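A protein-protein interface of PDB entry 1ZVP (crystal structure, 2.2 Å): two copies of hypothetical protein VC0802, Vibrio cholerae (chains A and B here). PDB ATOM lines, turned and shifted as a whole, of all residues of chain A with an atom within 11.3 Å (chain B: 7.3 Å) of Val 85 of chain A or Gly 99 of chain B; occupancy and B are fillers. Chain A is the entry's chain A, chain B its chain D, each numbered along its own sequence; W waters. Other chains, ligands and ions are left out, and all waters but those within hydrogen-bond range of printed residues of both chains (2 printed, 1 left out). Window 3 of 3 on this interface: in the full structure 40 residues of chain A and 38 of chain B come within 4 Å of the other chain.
Position printed for both chains: 93.
Of the 5 pairs that touch across the chains among the printed residues, none has its exchanged pair printed and touching as well.
Water W2 bridges the side-chain carboxylate of Asp 111 of chain A (2.7 Å) and the backbone carbonyl oxygen of Ala 102 of chain B (3.3 Å).
Water W1 lies within hydrogen-bond range of the side-chain hydroxyl (OG1) of Thr 93 of chain A (2.7 Å) and the side-chain hydroxyl (OG1) of Thr 93 of chain B (2.9 Å).
Val 85 of chain A touches Gly 99 of chain B (CG2 to CA, 3.8 Å).
OG of Ser 101 of chain B touches CG1 of Val 85 of chain A (3.8 Å).
Gly 86 of chain A touches Ala 96 of chain B (CA to CB, 3.9 Å).
Thr 88 of chain A touches Ala 102 of chain B (OG1 to O, 3.9 Å).
OG1 of Thr 93 of chain B touches CB of Ala 89 of chain A, 3.8 Å away.
The backbone carbonyl oxygen (O) of Gly 99 of chain B lies within hydrogen-bond range of the side-chain amino group (NZ) of Lys 119 of chain B (3.4 Å).
The backbone carbonyl oxygen of Ala 89 of chain A sits at hydrogen-bond distance from the side-chain hydroxyl of Thr 93 of chain A, at 2.5 Å.
Val 85 of chain A touches two residues of chain B.
Printed residues of chain B within 4 Å of Thr 88 of chain A: Ala 102.
Printed residues of chain B within 4 Å of Ala 89 of chain A: Thr 93.
Printed residues of chain A within 4 Å of Thr 93 of chain B: Ala 89.
Leu 95 of chain B touches none of the printed residues of chain A.
Gly 99 of chain B touches just one residue of chain A: Val 85.
No residue of chain A comes within 4 Å of Ile 100 of chain B.
Of the printed residues of chain A, Ala 102 of chain B touches Thr 88.
Gln 116 of chain B touches none of the printed residues of chain A.
The nearest residue of chain B that does not touch Val 85 of chain A is Ala 96 of chain B (4.1 Å).
The nearest residue of chain A that does not touch Gly 99 of chain B is Gly 86 of chain A (7.1 Å).
Of the 23 printed residues of chain A, 4 touch a printed residue of chain B.
Printed residues of chain A that touch a printed residue of chain B: Val 85, Gly 86, Thr 88 and Ala 89.
Hydrophobic or aromatic side chains of chain A that line the printed part of chain B: Val 85 and Ala 89.
Of the 12 printed residues of chain B, 5 touch a printed residue of chain A.
Printed residues of chain B that touch a printed residue of chain A: Thr 93, Ala 96, Gly 99, Ser 101 and Ala 102.
Hydrophobic or aromatic side chains of chain B that line the printed part of chain A: Ala 96.
Among the printed residues, 5 pairs touch across the chains.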
ATOM      1  N   SER A   3      -4.537   2.167 -25.979  1.00  0.00           N
ATOM      2  CA  SER A   3      -4.167   3.483 -25.371  1.00  0.00           C
ATOM      3  C   SER A   3      -4.376   3.491 -23.842  1.00  0.00           C
ATOM      4  O   SER A   3      -3.898   4.403 -23.150  1.00  0.00           O
ATOM      5  CB  SER A   3      -4.932   4.630 -26.054  1.00  0.00           C
ATOM      6  OG  SER A   3      -4.191   5.839 -26.021  1.00  0.00           O
ATOM      7  N   GLY A   4      -5.089   2.478 -23.334  1.00  0.00           N
ATOM      8  CA  GLY A   4      -5.199   2.213 -21.887  1.00  0.00           C
ATOM      9  C   GLY A   4      -4.038   1.358 -21.376  1.00  0.00           C
ATOM     10  O   GLY A   4      -3.631   1.470 -20.207  1.00  0.00           O
ATOM     11  N   ILE A   5      -3.522   0.502 -22.271  1.00  0.00           N
ATOM     12  CA  ILE A   5      -2.295  -0.298 -22.077  1.00  0.00           C
ATOM     13  C   ILE A   5      -1.067   0.584 -21.885  1.00  0.00           C
ATOM     14  O   ILE A   5      -0.398   0.539 -20.842  1.00  0.00           O
ATOM     15  CB  ILE A   5      -1.930  -1.153 -23.346  1.00  0.00           C
ATOM     16  CG1 ILE A   5      -3.154  -1.510 -24.209  1.00  0.00           C
ATOM     17  CG2 ILE A   5      -1.053  -2.344 -22.971  1.00  0.00           C
ATOM     18  CD1 ILE A   5      -3.227  -0.707 -25.510  1.00  0.00           C
ATOM     19  N   LYS A   6      -0.795   1.375 -22.930  1.00  0.00           N
ATOM     20  CA  LYS A   6       0.479   2.059 -23.129  1.00  0.00           C
ATOM     21  C   LYS A   6       0.615   3.348 -22.304  1.00  0.00           C
ATOM     22  O   LYS A   6       1.698   3.945 -22.240  1.00  0.00           O
ATOM     23  CB  LYS A   6       0.759   2.257 -24.644  1.00  0.00           C
ATOM     24  CG  LYS A   6       0.073   3.437 -25.340  1.00  0.00           C
ATOM     25  CD  LYS A   6       1.041   4.624 -25.462  1.00  0.00           C
ATOM     26  CE  LYS A   6       0.424   5.814 -26.189  1.00  0.00           C
ATOM     27  NZ  LYS A   6       0.463   5.650 -27.673  1.00  0.00           N
ATOM     28  N   SER A   7      -0.476   3.750 -21.656  1.00  0.00           N
ATOM     29  CA  SER A   7      -0.453   4.906 -20.769  1.00  0.00           C
ATOM     30  C   SER A   7       0.317   4.614 -19.470  1.00  0.00           C
ATOM     31  O   SER A   7       0.778   5.542 -18.807  1.00  0.00           O
ATOM     32  CB  SER A   7      -1.873   5.394 -20.469  1.00  0.00           C
ATOM     33  OG  SER A   7      -2.470   4.621 -19.445  1.00  0.00           O
ATOM     34  N   LEU A   8       0.456   3.332 -19.121  1.00  0.00           N
ATOM     35  CA  LEU A   8       1.282   2.918 -17.980  1.00  0.00           C
ATOM     36  C   LEU A   8       2.776   2.925 -18.320  1.00  0.00           C
ATOM     37  O   LEU A   8       3.608   3.324 -17.501  1.00  0.00           O
ATOM     38  CB  LEU A   8       0.857   1.540 -17.450  1.00  0.00           C
ATOM     39  CG  LEU A   8       1.704   0.895 -16.337  1.00  0.00           C
ATOM     40  CD1 LEU A   8       1.649   1.682 -15.026  1.00  0.00           C
ATOM     41  CD2 LEU A   8       1.294  -0.543 -16.125  1.00  0.00           C
ATOM     42  N   GLU A   9       3.105   2.483 -19.530  1.00  0.00           N
ATOM     43  CA  GLU A   9       4.484   2.481 -20.026  1.00  0.00           C
ATOM     44  C   GLU A   9       5.034   3.904 -20.148  1.00  0.00           C
ATOM     45  O   GLU A   9       6.226   4.137 -19.945  1.00  0.00           O
ATOM     46  CB  GLU A   9       4.553   1.734 -21.358  1.00  0.00           C
ATOM     47  CG  GLU A   9       3.884   0.353 -21.272  1.00  0.00           C
ATOM     48  CD  GLU A   9       3.516  -0.247 -22.619  1.00  0.00           C
ATOM     49  OE1 GLU A   9       2.612  -1.130 -22.644  1.00  0.00           O
ATOM     50  OE2 GLU A   9       4.132   0.159 -23.637  1.00  0.00           O
ATOM     51  N   LEU A  10       4.138   4.838 -20.466  1.00  0.00           N
ATOM     52  CA  LEU A  10       4.427   6.266 -20.492  1.00  0.00           C
ATOM     53  C   LEU A  10       4.690   6.816 -19.107  1.00  0.00           C
ATOM     54  O   LEU A  10       5.601   7.625 -18.923  1.00  0.00           O
ATOM     55  CB  LEU A  10       3.268   7.038 -21.134  1.00  0.00           C
ATOM     56  CG  LEU A  10       3.441   7.610 -22.547  1.00  0.00           C
ATOM     57  CD1 LEU A  10       4.269   6.709 -23.476  1.00  0.00           C
ATOM     58  CD2 LEU A  10       2.073   7.905 -23.157  1.00  0.00           C
ATOM     59  N   LEU A  11       3.887   6.378 -18.140  1.00  0.00           N
ATOM     60  CA  LEU A  11       4.038   6.804 -16.753  1.00  0.00           C
ATOM     61  C   LEU A  11       5.352   6.301 -16.162  1.00  0.00           C
ATOM     62  O   LEU A  11       6.038   7.027 -15.438  1.00  0.00           O
ATOM     63  CB  LEU A  11       2.859   6.315 -15.912  1.00  0.00           C
ATOM     64  CG  LEU A  11       2.926   6.642 -14.418  1.00  0.00           C
ATOM     65  CD1 LEU A  11       2.454   8.074 -14.128  1.00  0.00           C
ATOM     66  CD2 LEU A  11       2.120   5.625 -13.635  1.00  0.00           C
ATOM     67  N   LEU A  12       5.696   5.057 -16.482  1.00  0.00           N
ATOM     68  CA  LEU A  12       6.923   4.437 -15.999  1.00  0.00           C
ATOM     69  C   LEU A  12       8.177   5.072 -16.589  1.00  0.00           C
ATOM     70  O   LEU A  12       9.190   5.160 -15.905  1.00  0.00           O
ATOM     71  CB  LEU A  12       6.915   2.930 -16.263  1.00  0.00           C
ATOM     72  CG  LEU A  12       5.872   2.063 -15.556  1.00  0.00           C
ATOM     73  CD1 LEU A  12       6.132   0.624 -15.906  1.00  0.00           C
ATOM     74  CD2 LEU A  12       5.874   2.256 -14.049  1.00  0.00           C
ATOM     75  N   VAL A  78       7.234  10.784 -10.348  1.00  0.00           N
ATOM     76  CA  VAL A  78       6.688  10.514 -11.681  1.00  0.00           C
ATOM     77  C   VAL A  78       6.286  11.835 -12.311  1.00  0.00           C
ATOM     78  O   VAL A  78       5.792  12.728 -11.618  1.00  0.00           O
ATOM     79  CB  VAL A  78       5.490   9.517 -11.674  1.00  0.00           C
ATOM     80  CG1 VAL A  78       5.989   8.092 -11.526  1.00  0.00           C
ATOM     81  CG2 VAL A  78       4.480   9.851 -10.583  1.00  0.00           C
ATOM     82  N   SER A  80       4.211  13.034 -15.486  1.00  0.00           N
ATOM     83  CA  SER A  80       3.429  12.680 -14.284  1.00  0.00           C
ATOM     84  C   SER A  80       2.091  12.045 -14.698  1.00  0.00           C
ATOM     85  O   SER A  80       1.376  12.567 -15.571  1.00  0.00           O
ATOM     86  CB  SER A  80       3.168  13.904 -13.386  1.00  0.00           C
ATOM     87  OG  SER A  80       2.347  13.559 -12.276  1.00  0.00           O
ATOM     88  N   GLU A  83      -1.379   9.800 -15.633  1.00  0.00           N
ATOM     89  CA  GLU A  83      -1.275   8.848 -14.517  1.00  0.00           C
ATOM     90  C   GLU A  83      -2.280   7.645 -14.599  1.00  0.00           C
ATOM     91  O   GLU A  83      -3.406   7.791 -15.103  1.00  0.00           O
ATOM     92  CB  GLU A  83      -1.312   9.586 -13.148  1.00  0.00           C
ATOM     93  CG  GLU A  83      -2.640   9.472 -12.303  1.00  0.00           C
ATOM     94  CD  GLU A  83      -3.760  10.462 -12.721  1.00  0.00           C
ATOM     95  OE1 GLU A  83      -3.510  11.696 -12.726  1.00  0.00           O
ATOM     96  OE2 GLU A  83      -4.893  10.000 -13.020  1.00  0.00           O
ATOM     97  N   ALA A  84      -1.845   6.475 -14.103  1.00  0.00           N
ATOM     98  CA  ALA A  84      -2.556   5.184 -14.231  1.00  0.00           C
ATOM     99  C   ALA A  84      -2.267   4.251 -13.028  1.00  0.00           C
ATOM    100  O   ALA A  84      -1.575   4.660 -12.075  1.00  0.00           O
ATOM    101  CB  ALA A  84      -2.170   4.502 -15.552  1.00  0.00           C
ATOM    102  N   VAL A  85      -2.796   3.015 -13.060  1.00  0.00           N
ATOM    103  CA  VAL A  85      -2.537   2.028 -11.981  1.00  0.00           C
ATOM    104  C   VAL A  85      -1.467   0.993 -12.361  1.00  0.00           C
ATOM    105  O   VAL A  85      -1.401   0.552 -13.507  1.00  0.00           O
ATOM    106  CB  VAL A  85      -3.828   1.318 -11.458  1.00  0.00           C
ATOM    107  CG1 VAL A  85      -4.981   2.286 -11.372  1.00  0.00           C
ATOM    108  CG2 VAL A  85      -4.209   0.164 -12.318  1.00  0.00           C
ATOM    109  N   GLY A  86      -0.628   0.624 -11.397  1.00  0.00           N
ATOM    110  CA  GLY A  86       0.459  -0.319 -11.639  1.00  0.00           C
ATOM    111  C   GLY A  86       1.851   0.206 -11.326  1.00  0.00           C
ATOM    112  O   GLY A  86       2.838  -0.507 -11.509  1.00  0.00           O
ATOM    113  N   LEU A  87       1.934   1.450 -10.855  1.00  0.00           N
ATOM    114  CA  LEU A  87       3.216   2.083 -10.557  1.00  0.00           C
ATOM    115  C   LEU A  87       3.993   1.345  -9.473  1.00  0.00           C
ATOM    116  O   LEU A  87       5.177   1.062  -9.659  1.00  0.00           O
ATOM    117  CB  LEU A  87       3.034   3.555 -10.161  1.00  0.00           C
ATOM    118  CG  LEU A  87       4.323   4.270  -9.721  1.00  0.00           C
ATOM    119  CD1 LEU A  87       5.278   4.524 -10.909  1.00  0.00           C
ATOM    120  CD2 LEU A  87       4.036   5.558  -8.947  1.00  0.00           C
ATOM    121  N   THR A  88       3.325   1.048  -8.351  1.00  0.00           N
ATOM    122  CA  THR A  88       3.944   0.342  -7.220  1.00  0.00           C
ATOM    123  C   THR A  88       4.367  -1.070  -7.609  1.00  0.00           C
ATOM    124  O   THR A  88       5.456  -1.513  -7.242  1.00  0.00           O
ATOM    125  CB  THR A  88       3.025   0.264  -5.969  1.00  0.00           C
ATOM    126  OG1 THR A  88       2.408   1.528  -5.727  1.00  0.00           O
ATOM    127  CG2 THR A  88       3.813  -0.145  -4.735  1.00  0.00           C
ATOM    128  N   ALA A  89       3.502  -1.770  -8.343  1.00  0.00           N
ATOM    129  CA  ALA A  89       3.816  -3.112  -8.821  1.00  0.00           C
ATOM    130  C   ALA A  89       5.093  -3.099  -9.659  1.00  0.00           C
ATOM    131  O   ALA A  89       5.963  -3.951  -9.481  1.00  0.00           O
ATOM    132  CB  ALA A  89       2.663  -3.674  -9.609  1.00  0.00           C
ATOM    133  N   ALA A  90       5.207  -2.107 -10.545  1.00  0.00           N
ATOM    134  CA  ALA A  90       6.359  -1.963 -11.447  1.00  0.00           C
ATOM    135  C   ALA A  90       7.687  -1.706 -10.739  1.00  0.00           C
ATOM    136  O   ALA A  90       8.656  -2.431 -10.974  1.00  0.00           O
ATOM    137  CB  ALA A  90       6.094  -0.892 -12.491  1.00  0.00           C
ATOM    138  N   PHE A  91       7.751  -0.696  -9.874  1.00  0.00           N
ATOM    139  CA  PHE A  91       9.027  -0.419  -9.230  1.00  0.00           C
ATOM    140  C   PHE A  91       9.430  -1.477  -8.211  1.00  0.00           C
ATOM    141  O   PHE A  91      10.618  -1.752  -8.057  1.00  0.00           O
ATOM    142  CB  PHE A  91       9.160   1.023  -8.705  1.00  0.00           C
ATOM    143  CG  PHE A  91       8.393   1.321  -7.445  1.00  0.00           C
ATOM    144  CD1 PHE A  91       8.779   0.777  -6.221  1.00  0.00           C
ATOM    145  CD2 PHE A  91       7.332   2.218  -7.467  1.00  0.00           C
ATOM    146  CE1 PHE A  91       8.078   1.073  -5.045  1.00  0.00           C
ATOM    147  CE2 PHE A  91       6.631   2.533  -6.302  1.00  0.00           C
ATOM    148  CZ  PHE A  91       7.004   1.959  -5.083  1.00  0.00           C
ATOM    149  N   THR A  93       8.547  -4.735  -8.436  1.00  0.00           N
ATOM    150  CA  THR A  93       8.963  -5.871  -9.262  1.00  0.00           C
ATOM    151  C   THR A  93      10.399  -5.707  -9.763  1.00  0.00           C
ATOM    152  O   THR A  93      11.179  -6.664  -9.714  1.00  0.00           O
ATOM    153  CB  THR A  93       8.003  -6.100 -10.465  1.00  0.00           C
ATOM    154  OG1 THR A  93       6.681  -6.339  -9.980  1.00  0.00           O
ATOM    155  CG2 THR A  93       8.424  -7.294 -11.302  1.00  0.00           C
ATOM    156  N   ASP A 111       5.995   8.683  -3.106  1.00  0.00           N
ATOM    157  CA  ASP A 111       6.325   7.368  -2.575  1.00  0.00           C
ATOM    158  C   ASP A 111       7.764   7.386  -2.062  1.00  0.00           C
ATOM    159  O   ASP A 111       8.662   7.892  -2.726  1.00  0.00           O
ATOM    160  CB  ASP A 111       6.214   6.319  -3.684  1.00  0.00           C
ATOM    161  CG  ASP A 111       4.858   5.621  -3.721  1.00  0.00           C
ATOM    162  OD1 ASP A 111       4.161   5.578  -2.685  1.00  0.00           O
ATOM    163  OD2 ASP A 111       4.504   5.092  -4.798  1.00  0.00           O
ATOM    164  N   THR B  93       1.058  -6.045  -7.107  1.00  0.00           N
ATOM    165  CA  THR B  93       0.598  -6.715  -8.331  1.00  0.00           C
ATOM    166  C   THR B  93      -0.837  -7.234  -8.239  1.00  0.00           C
ATOM    167  O   THR B  93      -1.604  -7.077  -9.195  1.00  0.00           O
ATOM    168  CB  THR B  93       1.528  -7.885  -8.734  1.00  0.00           C
ATOM    169  OG1 THR B  93       2.823  -7.373  -9.008  1.00  0.00           O
ATOM    170  CG2 THR B  93       1.029  -8.596  -9.983  1.00  0.00           C
ATOM    171  N   LYS B  94      -1.190  -7.865  -7.115  1.00  0.00           N
ATOM    172  CA  LYS B  94      -2.539  -8.386  -6.914  1.00  0.00           C
ATOM    173  C   LYS B  94      -3.584  -7.274  -6.993  1.00  0.00           C
ATOM    174  O   LYS B  94      -4.672  -7.469  -7.545  1.00  0.00           O
ATOM    175  CB  LYS B  94      -2.660  -9.053  -5.556  1.00  0.00           C
ATOM    176  CG  LYS B  94      -1.956 -10.357  -5.423  1.00  0.00           C
ATOM    177  CD  LYS B  94      -1.934 -10.739  -3.961  1.00  0.00           C
ATOM    178  CE  LYS B  94      -1.618 -12.186  -3.793  1.00  0.00           C
ATOM    179  NZ  LYS B  94      -2.808 -13.045  -3.999  1.00  0.00           N
ATOM    180  N   LEU B  95      -3.248  -6.125  -6.410  1.00  0.00           N
ATOM    181  CA  LEU B  95      -4.095  -4.941  -6.445  1.00  0.00           C
ATOM    182  C   LEU B  95      -4.185  -4.320  -7.845  1.00  0.00           C
ATOM    183  O   LEU B  95      -5.276  -3.985  -8.294  1.00  0.00           O
ATOM    184  CB  LEU B  95      -3.587  -3.910  -5.433  1.00  0.00           C
ATOM    185  CG  LEU B  95      -4.216  -3.637  -4.069  1.00  0.00           C
ATOM    186  CD1 LEU B  95      -5.253  -4.651  -3.675  1.00  0.00           C
ATOM    187  CD2 LEU B  95      -3.135  -3.546  -3.023  1.00  0.00           C
ATOM    188  N   ALA B  96      -3.047  -4.159  -8.523  1.00  0.00           N
ATOM    189  CA  ALA B  96      -3.015  -3.590  -9.866  1.00  0.00           C
ATOM    190  C   ALA B  96      -3.801  -4.420 -10.873  1.00  0.00           C
ATOM    191  O   ALA B  96      -4.438  -3.869 -11.761  1.00  0.00           O
ATOM    192  CB  ALA B  96      -1.576  -3.396 -10.339  1.00  0.00           C
ATOM    193  N   GLU B  97      -3.764  -5.741 -10.729  1.00  0.00           N
ATOM    194  CA  GLU B  97      -4.527  -6.639 -11.590  1.00  0.00           C
ATOM    195  C   GLU B  97      -6.028  -6.390 -11.565  1.00  0.00           C
ATOM    196  O   GLU B  97      -6.741  -6.795 -12.485  1.00  0.00           O
ATOM    197  CB  GLU B  97      -4.285  -8.091 -11.198  1.00  0.00           C
ATOM    198  CG  GLU B  97      -3.057  -8.693 -11.803  1.00  0.00           C
ATOM    199  CD  GLU B  97      -2.887 -10.141 -11.400  1.00  0.00           C
ATOM    200  OE1 GLU B  97      -3.482 -11.025 -12.061  1.00  0.00           O
ATOM    201  OE2 GLU B  97      -2.148 -10.392 -10.419  1.00  0.00           O
ATOM    202  N   HIS B  98      -6.509  -5.761 -10.498  1.00  0.00           N
ATOM    203  CA  HIS B  98      -7.924  -5.412 -10.376  1.00  0.00           C
ATOM    204  C   HIS B  98      -8.206  -3.918 -10.502  1.00  0.00           C
ATOM    205  O   HIS B  98      -9.314  -3.464 -10.215  1.00  0.00           O
ATOM    206  CB  HIS B  98      -8.490  -5.978  -9.085  1.00  0.00           C
ATOM    207  CG  HIS B  98      -8.520  -7.467  -9.076  1.00  0.00           C
ATOM    208  ND1 HIS B  98      -7.451  -8.228  -8.660  1.00  0.00           N
ATOM    209  CD2 HIS B  98      -9.466  -8.339  -9.488  1.00  0.00           C
ATOM    210  CE1 HIS B  98      -7.749  -9.506  -8.786  1.00  0.00           C
ATOM    211  NE2 HIS B  98      -8.966  -9.601  -9.285  1.00  0.00           N
ATOM    212  N   GLY B  99      -7.201  -3.173 -10.956  1.00  0.00           N
ATOM    213  CA  GLY B  99      -7.326  -1.751 -11.202  1.00  0.00           C
ATOM    214  C   GLY B  99      -7.418  -0.924  -9.944  1.00  0.00           C
ATOM    215  O   GLY B  99      -8.075   0.113  -9.938  1.00  0.00           O
ATOM    216  N   ILE B 100      -6.749  -1.383  -8.888  1.00  0.00           N
ATOM    217  CA  ILE B 100      -6.755  -0.723  -7.580  1.00  0.00           C
ATOM    218  C   ILE B 100      -5.396  -0.091  -7.255  1.00  0.00           C
ATOM    219  O   ILE B 100      -4.368  -0.775  -7.198  1.00  0.00           O
ATOM    220  CB  ILE B 100      -7.178  -1.700  -6.455  1.00  0.00           C
ATOM    221  CG1 ILE B 100      -8.563  -2.271  -6.746  1.00  0.00           C
ATOM    222  CG2 ILE B 100      -7.150  -1.002  -5.096  1.00  0.00           C
ATOM    223  CD1 ILE B 100      -8.866  -3.562  -6.065  1.00  0.00           C
ATOM    224  N   SER B 101      -5.388   1.225  -7.057  1.00  0.00           N
ATOM    225  CA  SER B 101      -4.181   1.899  -6.612  1.00  0.00           C
ATOM    226  C   SER B 101      -4.013   1.833  -5.102  1.00  0.00           C
ATOM    227  O   SER B 101      -4.965   1.988  -4.343  1.00  0.00           O
ATOM    228  CB  SER B 101      -4.115   3.329  -7.118  1.00  0.00           C
ATOM    229  OG  SER B 101      -3.235   3.398  -8.228  1.00  0.00           O
ATOM    230  N   ALA B 102      -2.784   1.575  -4.680  1.00  0.00           N
ATOM    231  CA  ALA B 102      -2.465   1.384  -3.279  1.00  0.00           C
ATOM    232  C   ALA B 102      -1.498   2.447  -2.776  1.00  0.00           C
ATOM    233  O   ALA B 102      -0.486   2.745  -3.427  1.00  0.00           O
ATOM    234  CB  ALA B 102      -1.858  -0.001  -3.082  1.00  0.00           C
ATOM    235  N   GLN B 116      -8.787   3.431  -1.949  1.00  0.00           N
ATOM    236  CA  GLN B 116     -10.027   4.194  -2.019  1.00  0.00           C
ATOM    237  C   GLN B 116     -11.111   3.439  -1.304  1.00  0.00           C
ATOM    238  O   GLN B 116     -11.221   2.223  -1.456  1.00  0.00           O
ATOM    239  CB  GLN B 116     -10.445   4.398  -3.464  1.00  0.00           C
ATOM    240  CG  GLN B 116      -9.607   5.402  -4.210  1.00  0.00           C
ATOM    241  CD  GLN B 116      -9.897   5.385  -5.699  1.00  0.00           C
ATOM    242  OE1 GLN B 116      -9.205   6.036  -6.482  1.00  0.00           O
ATOM    243  NE2 GLN B 116     -10.921   4.637  -6.100  1.00  0.00           N
ATOM    244  N   LYS B 119     -13.372   0.946  -3.057  1.00  0.00           N
ATOM    245  CA  LYS B 119     -12.701  -0.241  -3.553  1.00  0.00           C
ATOM    246  C   LYS B 119     -12.210  -1.179  -2.449  1.00  0.00           C
ATOM    247  O   LYS B 119     -11.460  -2.112  -2.718  1.00  0.00           O
ATOM    248  CB  LYS B 119     -11.564   0.174  -4.486  1.00  0.00           C
ATOM    249  CG  LYS B 119     -12.062   0.536  -5.868  1.00  0.00           C
ATOM    250  CD  LYS B 119     -11.001   1.238  -6.662  1.00  0.00           C
ATOM    251  CE  LYS B 119     -11.456   1.445  -8.098  1.00  0.00           C
ATOM    252  NZ  LYS B 119     -10.466   2.265  -8.853  1.00  0.00           N
HETATM  253  O   HOH W   1       5.148  -8.594 -10.158  1.00  0.00           O
HETATM  254  O   HOH W   2       2.385   3.679  -2.043  1.00  0.00           O
